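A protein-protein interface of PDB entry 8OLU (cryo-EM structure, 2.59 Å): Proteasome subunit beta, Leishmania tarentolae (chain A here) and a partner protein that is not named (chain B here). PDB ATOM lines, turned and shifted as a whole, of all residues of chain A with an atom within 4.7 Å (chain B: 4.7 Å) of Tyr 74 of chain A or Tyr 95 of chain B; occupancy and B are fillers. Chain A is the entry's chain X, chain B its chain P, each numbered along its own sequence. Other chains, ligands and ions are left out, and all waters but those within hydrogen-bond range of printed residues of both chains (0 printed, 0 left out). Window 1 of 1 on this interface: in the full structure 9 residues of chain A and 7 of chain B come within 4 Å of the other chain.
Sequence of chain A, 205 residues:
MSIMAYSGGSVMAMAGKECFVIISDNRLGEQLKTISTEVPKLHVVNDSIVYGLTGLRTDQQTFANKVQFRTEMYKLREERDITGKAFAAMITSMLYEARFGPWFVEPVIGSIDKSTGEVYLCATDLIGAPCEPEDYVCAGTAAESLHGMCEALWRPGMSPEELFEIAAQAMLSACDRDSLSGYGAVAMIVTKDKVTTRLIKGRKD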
ATOM      1  N   ARG A  70      29.889  -1.539 -10.704  1.00  0.00           N
ATOM      2  CA  ARG A  70      29.076  -2.685 -10.449  1.00  0.00           C
ATOM      3  C   ARG A  70      29.840  -3.891  -9.972  1.00  0.00           C
ATOM      4  O   ARG A  70      29.368  -4.581  -9.095  1.00  0.00           O
ATOM      5  CB  ARG A  70      28.414  -3.135 -11.730  1.00  0.00           C
ATOM      6  CG  ARG A  70      27.329  -2.207 -12.239  1.00  0.00           C
ATOM      7  CD  ARG A  70      26.452  -1.677 -11.144  1.00  0.00           C
ATOM      8  NE  ARG A  70      25.469  -2.715 -10.830  1.00  0.00           N
ATOM      9  CZ  ARG A  70      24.497  -3.103 -11.666  1.00  0.00           C
ATOM     10  NH1 ARG A  70      24.097  -2.369 -12.718  1.00  0.00           N
ATOM     11  NH2 ARG A  70      23.993  -4.283 -11.407  1.00  0.00           N
ATOM     12  N   THR A  71      30.939  -4.202 -10.593  1.00  0.00           N
ATOM     13  CA  THR A  71      31.594  -5.401 -10.161  1.00  0.00           C
ATOM     14  C   THR A  71      32.325  -5.228  -8.864  1.00  0.00           C
ATOM     15  O   THR A  71      32.460  -6.201  -8.177  1.00  0.00           O
ATOM     16  CB  THR A  71      32.607  -5.943 -11.160  1.00  0.00           C
ATOM     17  OG1 THR A  71      33.553  -4.947 -11.535  1.00  0.00           O
ATOM     18  CG2 THR A  71      31.896  -6.449 -12.383  1.00  0.00           C
ATOM     19  N   GLU A  72      32.894  -4.064  -8.605  1.00  0.00           N
ATOM     20  CA  GLU A  72      33.623  -3.856  -7.377  1.00  0.00           C
ATOM     21  C   GLU A  72      32.650  -3.745  -6.225  1.00  0.00           C
ATOM     22  O   GLU A  72      32.909  -4.256  -5.151  1.00  0.00           O
ATOM     23  CB  GLU A  72      34.468  -2.595  -7.395  1.00  0.00           C
ATOM     24  CG  GLU A  72      35.704  -2.646  -8.308  1.00  0.00           C
ATOM     25  CD  GLU A  72      36.859  -3.614  -7.988  1.00  0.00           C
ATOM     26  OE1 GLU A  72      37.824  -3.646  -8.832  1.00  0.00           O
ATOM     27  OE2 GLU A  72      36.823  -4.361  -6.919  1.00  0.00           O
ATOM     28  N   MET A  73      31.487  -3.192  -6.505  1.00  0.00           N
ATOM     29  CA  MET A  73      30.453  -3.102  -5.514  1.00  0.00           C
ATOM     30  C   MET A  73      29.929  -4.472  -5.153  1.00  0.00           C
ATOM     31  O   MET A  73      29.840  -4.843  -4.035  1.00  0.00           O
ATOM     32  CB  MET A  73      29.352  -2.226  -6.059  1.00  0.00           C
ATOM     33  CG  MET A  73      28.284  -1.925  -5.031  1.00  0.00           C
ATOM     34  SD  MET A  73      28.716  -1.217  -3.345  1.00  0.00           S
ATOM     35  CE  MET A  73      29.675   0.109  -4.062  1.00  0.00           C
ATOM     36  N   TYR A  74      29.668  -5.257  -6.143  1.00  0.00           N
ATOM     37  CA  TYR A  74      29.292  -6.630  -6.008  1.00  0.00           C
ATOM     38  C   TYR A  74      30.224  -7.369  -5.102  1.00  0.00           C
ATOM     39  O   TYR A  74      29.782  -8.045  -4.224  1.00  0.00           O
ATOM     40  CB  TYR A  74      29.385  -7.311  -7.355  1.00  0.00           C
ATOM     41  CG  TYR A  74      28.858  -8.708  -7.391  1.00  0.00           C
ATOM     42  CD1 TYR A  74      29.645  -9.794  -7.059  1.00  0.00           C
ATOM     43  CD2 TYR A  74      27.550  -8.949  -7.722  1.00  0.00           C
ATOM     44  CE1 TYR A  74      29.152 -11.079  -7.035  1.00  0.00           C
ATOM     45  CE2 TYR A  74      27.049 -10.237  -7.737  1.00  0.00           C
ATOM     46  CZ  TYR A  74      27.851 -11.298  -7.384  1.00  0.00           C
ATOM     47  OH  TYR A  74      27.339 -12.563  -7.491  1.00  0.00           O
ATOM     48  N   LYS A  75      31.495  -7.232  -5.331  1.00  0.00           N
ATOM     49  CA  LYS A  75      32.504  -7.982  -4.620  1.00  0.00           C
ATOM     50  C   LYS A  75      32.569  -7.524  -3.176  1.00  0.00           C
ATOM     51  O   LYS A  75      32.867  -8.310  -2.298  1.00  0.00           O
ATOM     52  CB  LYS A  75      33.772  -7.843  -5.470  1.00  0.00           C
ATOM     53  CG  LYS A  75      35.087  -8.024  -4.778  1.00  0.00           C
ATOM     54  CD  LYS A  75      35.746  -9.304  -5.102  1.00  0.00           C
ATOM     55  CE  LYS A  75      37.048  -9.479  -4.348  1.00  0.00           C
ATOM     56  NZ  LYS A  75      37.336 -10.925  -4.156  1.00  0.00           N
ATOM     57  N   LEU A  76      32.264  -6.278  -2.888  1.00  0.00           N
ATOM     58  CA  LEU A  76      32.221  -5.871  -1.501  1.00  0.00           C
ATOM     59  C   LEU A  76      30.971  -6.353  -0.790  1.00  0.00           C
ATOM     60  O   LEU A  76      31.026  -6.783   0.347  1.00  0.00           O
ATOM     61  CB  LEU A  76      32.226  -4.356  -1.424  1.00  0.00           C
ATOM     62  CG  LEU A  76      33.566  -3.706  -1.726  1.00  0.00           C
ATOM     63  CD1 LEU A  76      33.397  -2.246  -2.087  1.00  0.00           C
ATOM     64  CD2 LEU A  76      34.498  -3.814  -0.572  1.00  0.00           C
ATOM     65  N   ARG A  77      29.812  -6.115  -1.385  1.00  0.00           N
ATOM     66  CA  ARG A  77      28.581  -6.533  -0.774  1.00  0.00           C
ATOM     67  C   ARG A  77      28.560  -8.042  -0.573  1.00  0.00           C
ATOM     68  O   ARG A  77      28.110  -8.544   0.444  1.00  0.00           O
ATOM     69  CB  ARG A  77      27.409  -6.235  -1.674  1.00  0.00           C
ATOM     70  CG  ARG A  77      26.997  -4.794  -1.742  1.00  0.00           C
ATOM     71  CD  ARG A  77      25.631  -4.792  -2.427  1.00  0.00           C
ATOM     72  NE  ARG A  77      25.137  -3.414  -2.358  1.00  0.00           N
ATOM     73  CZ  ARG A  77      25.194  -2.564  -3.389  1.00  0.00           C
ATOM     74  NH1 ARG A  77      25.389  -3.033  -4.620  1.00  0.00           N
ATOM     75  NH2 ARG A  77      25.030  -1.260  -3.190  1.00  0.00           N
ATOM     76  N   GLU A  78      28.987  -8.766  -1.572  1.00  0.00           N
ATOM     77  CA  GLU A  78      28.771 -10.177  -1.630  1.00  0.00           C
ATOM     78  C   GLU A  78      29.960 -10.945  -1.112  1.00  0.00           C
ATOM     79  O   GLU A  78      29.846 -12.135  -0.850  1.00  0.00           O
ATOM     80  CB  GLU A  78      28.595 -10.624  -3.078  1.00  0.00           C
ATOM     81  CG  GLU A  78      27.321 -10.091  -3.735  1.00  0.00           C
ATOM     82  CD  GLU A  78      26.431 -11.098  -4.488  1.00  0.00           C
ATOM     83  OE1 GLU A  78      25.358 -10.649  -4.978  1.00  0.00           O
ATOM     84  OE2 GLU A  78      26.770 -12.334  -4.580  1.00  0.00           O
ATOM     85  N   GLU A  79      31.108 -10.313  -1.021  1.00  0.00           N
ATOM     86  CA  GLU A  79      32.286 -10.995  -0.507  1.00  0.00           C
ATOM     87  C   GLU A  79      32.543 -12.219  -1.361  1.00  0.00           C
ATOM     88  O   GLU A  79      32.883 -13.256  -0.881  1.00  0.00           O
ATOM     89  CB  GLU A  79      32.176 -11.281   0.981  1.00  0.00           C
ATOM     90  CG  GLU A  79      31.597 -10.095   1.693  1.00  0.00           C
ATOM     91  CD  GLU A  79      31.762  -9.871   3.196  1.00  0.00           C
ATOM     92  OE1 GLU A  79      31.351  -8.718   3.657  1.00  0.00           O
ATOM     93  OE2 GLU A  79      32.237 -10.822   3.939  1.00  0.00           O
ATOM     94  N   ARG A  80      32.417 -12.077  -2.657  1.00  0.00           N
ATOM     95  CA  ARG A  80      32.966 -13.087  -3.519  1.00  0.00           C
ATOM     96  C   ARG A  80      33.115 -12.471  -4.908  1.00  0.00           C
ATOM     97  O   ARG A  80      32.661 -11.385  -5.163  1.00  0.00           O
ATOM     98  CB  ARG A  80      32.050 -14.305  -3.598  1.00  0.00           C
ATOM     99  CG  ARG A  80      30.632 -13.986  -4.060  1.00  0.00           C
ATOM    100  CD  ARG A  80      29.780 -15.197  -4.416  1.00  0.00           C
ATOM    101  NE  ARG A  80      28.413 -14.767  -4.721  1.00  0.00           N
ATOM    102  CZ  ARG A  80      27.550 -15.417  -5.500  1.00  0.00           C
ATOM    103  NH1 ARG A  80      27.876 -16.603  -5.975  1.00  0.00           N
ATOM    104  NH2 ARG A  80      26.365 -14.888  -5.803  1.00  0.00           N
ATOM    105  N   ASP A  81      33.792 -13.177  -5.784  1.00  0.00           N
ATOM    106  CA  ASP A  81      33.927 -12.721  -7.128  1.00  0.00           C
ATOM    107  C   ASP A  81      32.640 -13.018  -7.869  1.00  0.00           C
ATOM    108  O   ASP A  81      32.113 -14.121  -7.759  1.00  0.00           O
ATOM    109  CB  ASP A  81      35.075 -13.458  -7.820  1.00  0.00           C
ATOM    110  CG  ASP A  81      36.470 -12.914  -7.508  1.00  0.00           C
ATOM    111  OD1 ASP A  81      36.610 -11.623  -7.378  1.00  0.00           O
ATOM    112  OD2 ASP A  81      37.440 -13.780  -7.461  1.00  0.00           O
ATOM    113  N   ILE A  82      32.220 -12.095  -8.718  1.00  0.00           N
ATOM    114  CA  ILE A  82      31.151 -12.399  -9.632  1.00  0.00           C
ATOM    115  C   ILE A  82      31.576 -13.519 -10.536  1.00  0.00           C
ATOM    116  O   ILE A  82      32.769 -13.716 -10.729  1.00  0.00           O
ATOM    117  CB  ILE A  82      30.720 -11.155 -10.402  1.00  0.00           C
ATOM    118  CG1 ILE A  82      29.350 -11.349 -11.046  1.00  0.00           C
ATOM    119  CG2 ILE A  82      31.757 -10.692 -11.394  1.00  0.00           C
ATOM    120  CD1 ILE A  82      28.574 -10.047 -11.188  1.00  0.00           C
ATOM    121  N   ALA A  86      26.547 -14.593 -13.856  1.00  0.00           N
ATOM    122  CA  ALA A  86      26.020 -13.405 -13.219  1.00  0.00           C
ATOM    123  C   ALA A  86      26.499 -12.175 -13.949  1.00  0.00           C
ATOM    124  O   ALA A  86      25.730 -11.241 -14.174  1.00  0.00           O
ATOM    125  CB  ALA A  86      26.483 -13.331 -11.824  1.00  0.00           C
ATOM    126  N   ASN B  91      12.972  -8.969  -3.427  1.00  0.00           N
ATOM    127  CA  ASN B  91      14.388  -8.812  -3.547  1.00  0.00           C
ATOM    128  C   ASN B  91      14.978 -10.066  -4.134  1.00  0.00           C
ATOM    129  O   ASN B  91      15.873  -9.995  -4.958  1.00  0.00           O
ATOM    130  CB  ASN B  91      15.084  -8.612  -2.209  1.00  0.00           C
ATOM    131  CG  ASN B  91      14.787  -7.274  -1.573  1.00  0.00           C
ATOM    132  OD1 ASN B  91      14.753  -6.265  -2.260  1.00  0.00           O
ATOM    133  ND2 ASN B  91      14.612  -7.246  -0.260  1.00  0.00           N
ATOM    134  N   CYS B  92      14.551 -11.214  -3.653  1.00  0.00           N
ATOM    135  CA  CYS B  92      14.985 -12.426  -4.299  1.00  0.00           C
ATOM    136  C   CYS B  92      14.769 -12.387  -5.798  1.00  0.00           C
ATOM    137  O   CYS B  92      15.537 -12.982  -6.521  1.00  0.00           O
ATOM    138  CB  CYS B  92      14.188 -13.621  -3.828  1.00  0.00           C
ATOM    139  SG  CYS B  92      14.510 -14.026  -2.106  1.00  0.00           S
ATOM    140  N   GLN B  93      13.632 -11.872  -6.241  1.00  0.00           N
ATOM    141  CA  GLN B  93      13.306 -11.908  -7.635  1.00  0.00           C
ATOM    142  C   GLN B  93      14.091 -10.811  -8.340  1.00  0.00           C
ATOM    143  O   GLN B  93      14.522 -11.025  -9.455  1.00  0.00           O
ATOM    144  CB  GLN B  93      11.812 -11.758  -7.902  1.00  0.00           C
ATOM    145  CG  GLN B  93      10.961 -13.001  -7.672  1.00  0.00           C
ATOM    146  CD  GLN B  93      11.357 -14.187  -8.498  1.00  0.00           C
ATOM    147  OE1 GLN B  93      11.611 -14.092  -9.705  1.00  0.00           O
ATOM    148  NE2 GLN B  93      11.506 -15.324  -7.836  1.00  0.00           N
ATOM    149  N   GLN B  94      14.241  -9.632  -7.750  1.00  0.00           N
ATOM    150  CA  GLN B  94      15.015  -8.608  -8.407  1.00  0.00           C
ATOM    151  C   GLN B  94      16.410  -9.096  -8.665  1.00  0.00           C
ATOM    152  O   GLN B  94      16.947  -8.875  -9.726  1.00  0.00           O
ATOM    153  CB  GLN B  94      15.122  -7.324  -7.618  1.00  0.00           C
ATOM    154  CG  GLN B  94      13.801  -6.576  -7.652  1.00  0.00           C
ATOM    155  CD  GLN B  94      13.961  -5.300  -6.861  1.00  0.00           C
ATOM    156  OE1 GLN B  94      14.545  -4.330  -7.364  1.00  0.00           O
ATOM    157  NE2 GLN B  94      13.532  -5.323  -5.594  1.00  0.00           N
ATOM    158  N   TYR B  95      16.956  -9.812  -7.724  1.00  0.00           N
ATOM    159  CA  TYR B  95      18.291 -10.309  -7.849  1.00  0.00           C
ATOM    160  C   TYR B  95      18.365 -11.316  -8.961  1.00  0.00           C
ATOM    161  O   TYR B  95      19.344 -11.392  -9.630  1.00  0.00           O
ATOM    162  CB  TYR B  95      18.674 -10.969  -6.539  1.00  0.00           C
ATOM    163  CG  TYR B  95      20.122 -11.284  -6.429  1.00  0.00           C
ATOM    164  CD1 TYR B  95      21.029 -10.476  -5.781  1.00  0.00           C
ATOM    165  CD2 TYR B  95      20.603 -12.432  -7.020  1.00  0.00           C
ATOM    166  CE1 TYR B  95      22.366 -10.826  -5.715  1.00  0.00           C
ATOM    167  CE2 TYR B  95      21.926 -12.830  -6.880  1.00  0.00           C
ATOM    168  CZ  TYR B  95      22.815 -12.024  -6.213  1.00  0.00           C
ATOM    169  OH  TYR B  95      24.102 -12.535  -6.246  1.00  0.00           O
ATOM    170  N   LYS B  96      17.424 -12.226  -9.077  1.00  0.00           N
ATOM    171  CA  LYS B  96      17.467 -13.149 -10.181  1.00  0.00           C
ATOM    172  C   LYS B  96      17.355 -12.407 -11.488  1.00  0.00           C
ATOM    173  O   LYS B  96      17.968 -12.753 -12.465  1.00  0.00           O
ATOM    174  CB  LYS B  96      16.288 -14.089 -10.116  1.00  0.00           C
ATOM    175  CG  LYS B  96      16.674 -15.524  -9.940  1.00  0.00           C
ATOM    176  CD  LYS B  96      15.606 -16.318  -9.228  1.00  0.00           C
ATOM    177  CE  LYS B  96      16.051 -17.742  -8.970  1.00  0.00           C
ATOM    178  NZ  LYS B  96      15.331 -18.314  -7.805  1.00  0.00           N
ATOM    179  N   LEU B  97      16.471 -11.450 -11.555  1.00  0.00           N
ATOM    180  CA  LEU B  97      16.362 -10.724 -12.776  1.00  0.00           C
ATOM    181  C   LEU B  97      17.688 -10.103 -13.121  1.00  0.00           C
ATOM    182  O   LEU B  97      17.983  -9.964 -14.291  1.00  0.00           O
ATOM    183  CB  LEU B  97      15.359  -9.597 -12.653  1.00  0.00           C
ATOM    184  CG  LEU B  97      13.914 -10.013 -12.848  1.00  0.00           C
ATOM    185  CD1 LEU B  97      13.049  -8.794 -12.633  1.00  0.00           C
ATOM    186  CD2 LEU B  97      13.655 -10.585 -14.222  1.00  0.00           C
ATOM    187  N   MET B  98      18.438  -9.641 -12.138  1.00  0.00           N
ATOM    188  CA  MET B  98      19.692  -9.036 -12.489  1.00  0.00           C
ATOM    189  C   MET B  98      20.768 -10.076 -12.758  1.00  0.00           C
ATOM    190  O   MET B  98      21.407 -10.023 -13.762  1.00  0.00           O
ATOM    191  CB  MET B  98      20.200  -8.079 -11.444  1.00  0.00           C
ATOM    192  CG  MET B  98      21.312  -7.206 -12.011  1.00  0.00           C
ATOM    193  SD  MET B  98      21.500  -5.901 -10.827  1.00  0.00           S
ATOM    194  CE  MET B  98      20.046  -4.909 -11.173  1.00  0.00           C
ATOM    195  N   TYR B  99      21.011 -10.974 -11.876  1.00  0.00           N
ATOM    196  CA  TYR B  99      22.175 -11.783 -11.992  1.00  0.00           C
ATOM    197  C   TYR B  99      21.851 -13.171 -12.457  1.00  0.00           C
ATOM    198  O   TYR B  99      22.745 -13.952 -12.626  1.00  0.00           O
ATOM    199  CB  TYR B  99      22.875 -11.875 -10.653  1.00  0.00           C
ATOM    200  CG  TYR B  99      23.344 -10.542 -10.189  1.00  0.00           C
ATOM    201  CD1 TYR B  99      24.365  -9.879 -10.811  1.00  0.00           C
ATOM    202  CD2 TYR B  99      22.747  -9.927  -9.114  1.00  0.00           C
ATOM    203  CE1 TYR B  99      24.831  -8.655 -10.345  1.00  0.00           C
ATOM    204  CE2 TYR B  99      23.158  -8.691  -8.658  1.00  0.00           C
ATOM    205  CZ  TYR B  99      24.232  -8.068  -9.249  1.00  0.00           C
ATOM    206  OH  TYR B  99      24.496  -6.817  -8.805  1.00  0.00           O
ATOM    207  N   ASN B 100      20.580 -13.511 -12.559  1.00  0.00           N
ATOM    208  CA  ASN B 100      20.140 -14.742 -13.199  1.00  0.00           C
ATOM    209  C   ASN B 100      20.684 -15.924 -12.424  1.00  0.00           C
ATOM    210  O   ASN B 100      20.838 -16.984 -12.962  1.00  0.00           O
ATOM    211  CB  ASN B 100      20.472 -14.678 -14.694  1.00  0.00           C
ATOM    212  CG  ASN B 100      20.281 -15.979 -15.421  1.00  0.00           C
ATOM    213  OD1 ASN B 100      21.235 -16.515 -15.996  1.00  0.00           O
ATOM    214  ND2 ASN B 100      19.066 -16.505 -15.371  1.00  0.00           N
ATOM    215  N   GLU B 101      20.926 -15.691 -11.152  1.00  0.00           N
ATOM    216  CA  GLU B 101      21.328 -16.667 -10.161  1.00  0.00           C
ATOM    217  C   GLU B 101      20.424 -16.425  -8.960  1.00  0.00           C
ATOM    218  O   GLU B 101      19.981 -15.311  -8.807  1.00  0.00           O
ATOM    219  CB  GLU B 101      22.627 -16.298  -9.453  1.00  0.00           C
ATOM    220  CG  GLU B 101      23.931 -16.676 -10.100  1.00  0.00           C
ATOM    221  CD  GLU B 101      25.094 -16.256  -9.196  1.00  0.00           C
ATOM    222  OE1 GLU B 101      26.289 -16.647  -9.487  1.00  0.00           O
ATOM    223  OE2 GLU B 101      24.810 -15.512  -8.191  1.00  0.00           O
ATOM    224  N   PRO B 102      20.247 -17.344  -8.015  1.00  0.00           N
ATOM    225  CA  PRO B 102      19.601 -17.052  -6.762  1.00  0.00           C
ATOM    226  C   PRO B 102      20.332 -16.178  -5.749  1.00  0.00           C
ATOM    227  O   PRO B 102      21.471 -16.435  -5.377  1.00  0.00           O
ATOM    228  CB  PRO B 102      19.561 -18.371  -6.009  1.00  0.00           C
ATOM    229  CG  PRO B 102      20.000 -19.429  -6.993  1.00  0.00           C
ATOM    230  CD  PRO B 102      20.657 -18.722  -8.135  1.00  0.00           C
ATOM    231  N   ILE B 103      19.595 -15.246  -5.157  1.00  0.00           N
ATOM    232  CA  ILE B 103      20.195 -14.392  -4.155  1.00  0.00           C
ATOM    233  C   ILE B 103      20.790 -15.217  -3.035  1.00  0.00           C
ATOM    234  O   ILE B 103      20.157 -16.112  -2.531  1.00  0.00           O
ATOM    235  CB  ILE B 103      19.176 -13.403  -3.616  1.00  0.00           C
ATOM    236  CG1 ILE B 103      19.911 -12.215  -3.059  1.00  0.00           C
ATOM    237  CG2 ILE B 103      18.257 -14.054  -2.599  1.00  0.00           C
ATOM    238  CD1 ILE B 103      18.978 -11.177  -2.431  1.00  0.00           C
ATOM    239  N   PRO B 104      22.077 -15.038  -2.730  1.00  0.00           N
ATOM    240  CA  PRO B 104      22.707 -15.641  -1.579  1.00  0.00           C
ATOM    241  C   PRO B 104      22.081 -15.156  -0.311  1.00  0.00           C
ATOM    242  O   PRO B 104      21.760 -14.010  -0.253  1.00  0.00           O
ATOM    243  CB  PRO B 104      24.119 -15.077  -1.543  1.00  0.00           C
ATOM    244  CG  PRO B 104      24.374 -14.541  -2.878  1.00  0.00           C
ATOM    245  CD  PRO B 104      23.062 -14.355  -3.554  1.00  0.00           C
ATOM    246  N   LYS B 111      19.543  -7.235   3.001  1.00  0.00           N
ATOM    247  CA  LYS B 111      18.462  -6.468   2.448  1.00  0.00           C
ATOM    248  C   LYS B 111      17.325  -6.321   3.426  1.00  0.00           C
ATOM    249  O   LYS B 111      16.767  -5.231   3.504  1.00  0.00           O
ATOM    250  CB  LYS B 111      17.983  -7.056   1.136  1.00  0.00           C
ATOM    251  CG  LYS B 111      18.771  -6.459   0.001  1.00  0.00           C
ATOM    252  CD  LYS B 111      18.818  -7.225  -1.295  1.00  0.00           C
ATOM    253  CE  LYS B 111      19.598  -6.438  -2.336  1.00  0.00           C
ATOM    254  NZ  LYS B 111      20.563  -7.348  -2.996  1.00  0.00           N
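OH of Tyr 74 of chain A is in hydrogen-bond range of OE2 of Glu 78 of chain A (3.0 Å). The side-chain hydroxyl of Tyr 74 of chain A lies within hydrogen-bond range of the guanidinium group of Arg 80 of chain A, 3.0 Å away. The side-chain carboxylate (OE2) of Glu 78 of chain A lies within salt-bridge range of the guanidinium group (NH2) of Arg 80 of chain A (2.9 Å). The side-chain sulfur (SD) of Met 98 of chain B lies within hydrogen-bond range of the side-chain hydroxyl (OH) of Tyr 99 of chain B, at 3.7 Å.
Among the printed residues, pairs that only touch across the chains: Arg 70 of chain A with Tyr 99 of chain B (3.7 Å), Tyr 74 of chain A with Tyr 99 of chain B (3.8 Å), Tyr 74 of chain A with Glu 101 of chain B (3.9 Å), Glu 78 of chain A with Pro 104 of chain B (3.7 Å), Arg 80 of chain A with Pro 104 of chain B (3.6 Å) and Ala 86 of chain A with Tyr 99 of chain B (3.4 Å).
Of the 14 printed residues of chain A, 5 touch a printed residue of chain B. Printed residues of chain A that touch a printed residue of chain B: Arg 70, Tyr 74, Glu 78, Arg 80 and Ala 86. Hydrophobic or aromatic side chains of chain A within 4 Å of the printed part of chain B: Tyr 74 and Ala 86. Along chain B the printed residues that touch a printed residue of chain A span positions 95 to 104. Among the printed residues, 11 pairs touch across the chains.
Of chain B, only Tyr 95, Tyr 99 and Glu 101 come within 4 Å of Tyr 74 of chain A. Leu 76 of chain A touches none of the printed residues of chain B. Of the printed residues of chain B, Ala 86 of chain A touches Tyr 99. Of the printed residues of chain A, Tyr 95 of chain B touches Tyr 74, Glu 78 and Arg 80. Leu 97 of chain B touches none of the printed residues of chain A. Of the printed residues of chain A, Met 98 of chain B touches Arg 70. Of the printed residues of chain A, Glu 101 of chain B touches Tyr 74 (3.9 Å) and Arg 80 (2.9 Å). The nearest printed residue of chain A that does not touch Tyr 95 of chain B is Ala 86 of chain A (6.1 Å). The nearest printed residue of chain B that does not touch Ala 86 of chain A is Glu 101 of chain B (4.1 Å).
The side-chain sulfur (SD) of Met 98 of chain B lies within hydrogen-bond range of the guanidinium group (NH2) of Arg 70 of chain A, at 3.0 Å. OH of Tyr 95 of chain B is in hydrogen-bond range of OH of Tyr 74 of chain A, 3.5 Å away. The side-chain carboxylate of Glu 78 of chain A is in hydrogen-bond range of the side-chain hydroxyl of Tyr 95 of chain B. The guanidinium group (NH2) of Arg 80 of chain A sits at hydrogen-bond distance from the side-chain hydroxyl (OH) of Tyr 95 of chain B, at 3.3 Å. NH2 of Arg 80 of chain A lies within salt-bridge range of OE2 of Glu 101 of chain B, 2.9 Å away.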
